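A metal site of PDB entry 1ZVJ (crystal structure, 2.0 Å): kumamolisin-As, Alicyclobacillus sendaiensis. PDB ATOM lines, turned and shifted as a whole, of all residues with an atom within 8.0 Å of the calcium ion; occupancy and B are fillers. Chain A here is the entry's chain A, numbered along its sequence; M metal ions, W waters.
The side-chain carboxylate (OD1) of Asp 338 is in hydrogen-bond range of the side-chain hydroxyl (OG1) of Thr 341, at 2.7 Å. OD1 of Asp 338 sits at hydrogen-bond distance from N of Cys 340 (2.9 Å).
Water W1 lies within hydrogen-bond range of the side-chain hydroxyl (OG1) of Thr 341 (2.7 Å), the backbone carbonyl oxygen (O) of Gly 342 (2.8 Å), the backbone NH (N) of Gly 344 (3.3 Å) and the backbone NH (N) of Ile 317 (3.5 Å).
Of the 20 residues printed, 5 come within 4 Å of the calcium ion.
The calcium ion is bound by O of Gly 334, OD1 of Asp 316, O of Ile 317, O of Gly 336, OD2 of Asp 338 and water W1.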
ATOM      1  N   VAL A 207      -3.931  -4.203   9.241  1.00  0.00           N
ATOM      2  CA  VAL A 207      -2.733  -5.001   9.507  1.00  0.00           C
ATOM      3  C   VAL A 207      -1.615  -4.625   8.546  1.00  0.00           C
ATOM      4  O   VAL A 207      -1.831  -4.552   7.333  1.00  0.00           O
ATOM      5  CB  VAL A 207      -3.003  -6.507   9.397  1.00  0.00           C
ATOM      6  CG1 VAL A 207      -1.766  -7.303   9.794  1.00  0.00           C
ATOM      7  CG2 VAL A 207      -4.187  -6.922  10.245  1.00  0.00           C
ATOM      8  N   HIS A 315      -8.239   2.021  19.478  1.00  0.00           N
ATOM      9  CA  HIS A 315      -8.743   1.946  18.119  1.00  0.00           C
ATOM     10  C   HIS A 315      -8.525   0.526  17.580  1.00  0.00           C
ATOM     11  O   HIS A 315      -7.408   0.082  17.311  1.00  0.00           O
ATOM     12  CB  HIS A 315      -8.049   2.969  17.207  1.00  0.00           C
ATOM     13  CG  HIS A 315      -8.630   2.938  15.826  1.00  0.00           C
ATOM     14  ND1 HIS A 315      -8.151   2.119  14.835  1.00  0.00           N
ATOM     15  CD2 HIS A 315      -9.657   3.626  15.277  1.00  0.00           C
ATOM     16  CE1 HIS A 315      -8.849   2.288  13.719  1.00  0.00           C
ATOM     17  NE2 HIS A 315      -9.770   3.205  13.968  1.00  0.00           N
ATOM     18  N   ASP A 316      -9.643  -0.176  17.443  1.00  0.00           N
ATOM     19  CA  ASP A 316      -9.684  -1.563  16.985  1.00  0.00           C
ATOM     20  C   ASP A 316      -9.307  -1.690  15.507  1.00  0.00           C
ATOM     21  O   ASP A 316      -9.916  -1.073  14.631  1.00  0.00           O
ATOM     22  CB  ASP A 316     -11.092  -2.118  17.216  1.00  0.00           C
ATOM     23  CG  ASP A 316     -11.168  -3.622  17.101  1.00  0.00           C
ATOM     24  OD1 ASP A 316     -10.124  -4.216  16.765  1.00  0.00           O
ATOM     25  OD2 ASP A 316     -12.232  -4.228  17.350  1.00  0.00           O
ATOM     26  N   ILE A 317      -8.298  -2.501  15.217  1.00  0.00           N
ATOM     27  CA  ILE A 317      -8.027  -2.906  13.842  1.00  0.00           C
ATOM     28  C   ILE A 317      -8.838  -4.160  13.549  1.00  0.00           C
ATOM     29  O   ILE A 317      -8.814  -5.104  14.335  1.00  0.00           O
ATOM     30  CB  ILE A 317      -6.542  -3.174  13.580  1.00  0.00           C
ATOM     31  CG1 ILE A 317      -5.694  -1.895  13.516  1.00  0.00           C
ATOM     32  CG2 ILE A 317      -6.360  -4.029  12.329  1.00  0.00           C
ATOM     33  CD1 ILE A 317      -5.357  -1.337  14.882  1.00  0.00           C
ATOM     34  N   THR A 318      -9.587  -4.195  12.440  1.00  0.00           N
ATOM     35  CA  THR A 318     -10.407  -5.389  12.240  1.00  0.00           C
ATOM     36  C   THR A 318     -10.149  -6.069  10.911  1.00  0.00           C
ATOM     37  O   THR A 318     -10.756  -7.105  10.627  1.00  0.00           O
ATOM     38  CB  THR A 318     -11.915  -5.051  12.229  1.00  0.00           C
ATOM     39  OG1 THR A 318     -12.074  -3.908  11.371  1.00  0.00           O
ATOM     40  CG2 THR A 318     -12.435  -4.679  13.614  1.00  0.00           C
ATOM     41  N   GLU A 319      -9.291  -5.481  10.095  1.00  0.00           N
ATOM     42  CA  GLU A 319      -9.172  -5.923   8.708  1.00  0.00           C
ATOM     43  C   GLU A 319      -7.726  -6.165   8.290  1.00  0.00           C
ATOM     44  O   GLU A 319      -6.844  -5.321   8.494  1.00  0.00           O
ATOM     45  CB  GLU A 319      -9.813  -4.867   7.808  1.00  0.00           C
ATOM     46  CG  GLU A 319      -9.396  -5.006   6.346  1.00  0.00           C
ATOM     47  CD  GLU A 319      -9.942  -3.866   5.498  1.00  0.00           C
ATOM     48  OE1 GLU A 319     -10.602  -2.988   6.089  1.00  0.00           O
ATOM     49  OE2 GLU A 319      -9.696  -3.883   4.276  1.00  0.00           O
ATOM     50  N   GLN A 332      -5.613 -13.667  11.202  1.00  0.00           N
ATOM     51  CA  GLN A 332      -6.523 -12.651  10.710  1.00  0.00           C
ATOM     52  C   GLN A 332      -6.906 -11.622  11.770  1.00  0.00           C
ATOM     53  O   GLN A 332      -7.046 -11.958  12.947  1.00  0.00           O
ATOM     54  CB  GLN A 332      -7.817 -13.302  10.209  1.00  0.00           C
ATOM     55  CG  GLN A 332      -8.200 -12.890   8.797  1.00  0.00           C
ATOM     56  CD  GLN A 332      -9.059 -13.963   8.142  1.00  0.00           C
ATOM     57  OE1 GLN A 332      -8.706 -14.531   7.106  1.00  0.00           O
ATOM     58  NE2 GLN A 332     -10.187 -14.260   8.767  1.00  0.00           N
ATOM     59  N   ALA A 333      -7.109 -10.375  11.357  1.00  0.00           N
ATOM     60  CA  ALA A 333      -7.577  -9.363  12.328  1.00  0.00           C
ATOM     61  C   ALA A 333      -9.080  -9.499  12.529  1.00  0.00           C
ATOM     62  O   ALA A 333      -9.793 -10.066  11.697  1.00  0.00           O
ATOM     63  CB  ALA A 333      -7.203  -7.973  11.862  1.00  0.00           C
ATOM     64  N   GLY A 334      -9.600  -8.994  13.643  1.00  0.00           N
ATOM     65  CA  GLY A 334     -11.048  -9.112  13.845  1.00  0.00           C
ATOM     66  C   GLY A 334     -11.522  -8.172  14.926  1.00  0.00           C
ATOM     67  O   GLY A 334     -10.736  -7.353  15.409  1.00  0.00           O
ATOM     68  N   PRO A 335     -12.787  -8.277  15.330  1.00  0.00           N
ATOM     69  CA  PRO A 335     -13.290  -7.410  16.402  1.00  0.00           C
ATOM     70  C   PRO A 335     -12.578  -7.731  17.715  1.00  0.00           C
ATOM     71  O   PRO A 335     -12.420  -8.908  18.048  1.00  0.00           O
ATOM     72  CB  PRO A 335     -14.771  -7.762  16.498  1.00  0.00           C
ATOM     73  CG  PRO A 335     -15.097  -8.531  15.253  1.00  0.00           C
ATOM     74  CD  PRO A 335     -13.829  -9.184  14.806  1.00  0.00           C
ATOM     75  N   GLY A 336     -12.154  -6.701  18.432  1.00  0.00           N
ATOM     76  CA  GLY A 336     -11.490  -6.857  19.717  1.00  0.00           C
ATOM     77  C   GLY A 336     -10.045  -7.323  19.543  1.00  0.00           C
ATOM     78  O   GLY A 336      -9.456  -7.047  18.485  1.00  0.00           O
ATOM     79  N   TRP A 337      -9.490  -7.987  20.540  1.00  0.00           N
ATOM     80  CA  TRP A 337      -8.139  -8.522  20.479  1.00  0.00           C
ATOM     81  C   TRP A 337      -8.016  -9.480  19.298  1.00  0.00           C
ATOM     82  O   TRP A 337      -8.925 -10.267  19.042  1.00  0.00           O
ATOM     83  CB  TRP A 337      -7.752  -9.281  21.758  1.00  0.00           C
ATOM     84  CG  TRP A 337      -6.299  -9.679  21.762  1.00  0.00           C
ATOM     85  CD1 TRP A 337      -5.269  -8.970  22.328  1.00  0.00           C
ATOM     86  CD2 TRP A 337      -5.703 -10.854  21.191  1.00  0.00           C
ATOM     87  NE1 TRP A 337      -4.079  -9.627  22.141  1.00  0.00           N
ATOM     88  CE2 TRP A 337      -4.315 -10.783  21.446  1.00  0.00           C
ATOM     89  CE3 TRP A 337      -6.201 -11.958  20.500  1.00  0.00           C
ATOM     90  CZ2 TRP A 337      -3.441 -11.782  21.027  1.00  0.00           C
ATOM     91  CZ3 TRP A 337      -5.337 -12.937  20.072  1.00  0.00           C
ATOM     92  CH2 TRP A 337      -3.958 -12.838  20.334  1.00  0.00           C
ATOM     93  N   ASP A 338      -6.883  -9.448  18.610  1.00  0.00           N
ATOM     94  CA  ASP A 338      -6.599 -10.444  17.585  1.00  0.00           C
ATOM     95  C   ASP A 338      -5.099 -10.697  17.506  1.00  0.00           C
ATOM     96  O   ASP A 338      -4.310  -9.892  18.008  1.00  0.00           O
ATOM     97  CB  ASP A 338      -7.161 -10.018  16.227  1.00  0.00           C
ATOM     98  CG  ASP A 338      -6.647  -8.698  15.709  1.00  0.00           C
ATOM     99  OD1 ASP A 338      -5.429  -8.574  15.471  1.00  0.00           O
ATOM    100  OD2 ASP A 338      -7.492  -7.785  15.549  1.00  0.00           O
ATOM    101  N   PRO A 339      -4.658 -11.784  16.890  1.00  0.00           N
ATOM    102  CA  PRO A 339      -3.219 -12.110  16.893  1.00  0.00           C
ATOM    103  C   PRO A 339      -2.460 -11.321  15.831  1.00  0.00           C
ATOM    104  O   PRO A 339      -1.372 -11.731  15.427  1.00  0.00           O
ATOM    105  CB  PRO A 339      -3.189 -13.607  16.584  1.00  0.00           C
ATOM    106  CG  PRO A 339      -4.615 -14.053  16.524  1.00  0.00           C
ATOM    107  CD  PRO A 339      -5.412 -12.822  16.150  1.00  0.00           C
ATOM    108  N   CYS A 340      -3.016 -10.186  15.387  1.00  0.00           N
ATOM    109  CA  CYS A 340      -2.286  -9.358  14.435  1.00  0.00           C
ATOM    110  C   CYS A 340      -1.888  -8.022  15.063  1.00  0.00           C
ATOM    111  O   CYS A 340      -0.769  -7.563  14.867  1.00  0.00           O
ATOM    112  CB  CYS A 340      -3.092  -9.111  13.161  1.00  0.00           C
ATOM    113  SG  CYS A 340      -3.354 -10.575  12.139  1.00  0.00           S
ATOM    114  N   THR A 341      -2.824  -7.438  15.805  1.00  0.00           N
ATOM    115  CA  THR A 341      -2.760  -6.116  16.381  1.00  0.00           C
ATOM    116  C   THR A 341      -3.142  -6.077  17.855  1.00  0.00           C
ATOM    117  O   THR A 341      -3.206  -4.996  18.441  1.00  0.00           O
ATOM    118  CB  THR A 341      -3.769  -5.170  15.685  1.00  0.00           C
ATOM    119  OG1 THR A 341      -5.032  -5.860  15.608  1.00  0.00           O
ATOM    120  CG2 THR A 341      -3.320  -4.853  14.266  1.00  0.00           C
ATOM    121  N   GLY A 342      -3.417  -7.234  18.437  1.00  0.00           N
ATOM    122  CA  GLY A 342      -3.812  -7.238  19.849  1.00  0.00           C
ATOM    123  C   GLY A 342      -5.061  -6.406  20.079  1.00  0.00           C
ATOM    124  O   GLY A 342      -6.048  -6.539  19.346  1.00  0.00           O
ATOM    125  N   LEU A 343      -5.019  -5.548  21.100  1.00  0.00           N
ATOM    126  CA  LEU A 343      -6.115  -4.661  21.449  1.00  0.00           C
ATOM    127  C   LEU A 343      -6.301  -3.535  20.447  1.00  0.00           C
ATOM    128  O   LEU A 343      -7.334  -2.855  20.450  1.00  0.00           O
ATOM    129  CB  LEU A 343      -5.866  -4.089  22.859  1.00  0.00           C
ATOM    130  CG  LEU A 343      -5.896  -5.132  23.974  1.00  0.00           C
ATOM    131  CD1 LEU A 343      -5.259  -4.601  25.248  1.00  0.00           C
ATOM    132  CD2 LEU A 343      -7.326  -5.586  24.248  1.00  0.00           C
ATOM    133  N   GLY A 344      -5.315  -3.322  19.576  1.00  0.00           N
ATOM    134  CA  GLY A 344      -5.379  -2.242  18.621  1.00  0.00           C
ATOM    135  C   GLY A 344      -4.389  -1.123  18.916  1.00  0.00           C
ATOM    136  O   GLY A 344      -3.469  -1.270  19.724  1.00  0.00           O
ATOM    137  N   SER A 345      -4.580   0.025  18.261  1.00  0.00           N
ATOM    138  CA  SER A 345      -3.745   1.203  18.499  1.00  0.00           C
ATOM    139  C   SER A 345      -4.318   1.937  19.706  1.00  0.00           C
ATOM    140  O   SER A 345      -5.521   2.163  19.775  1.00  0.00           O
ATOM    141  CB  SER A 345      -3.681   2.112  17.272  1.00  0.00           C
ATOM    142  OG  SER A 345      -4.913   2.776  17.063  1.00  0.00           O
HETATM  143 CA    CA M   1      -8.987  -6.195  16.371  1.00  0.00          CA
HETATM  144  O   HOH W   1      -7.018  -4.997  17.252  1.00  0.00           O
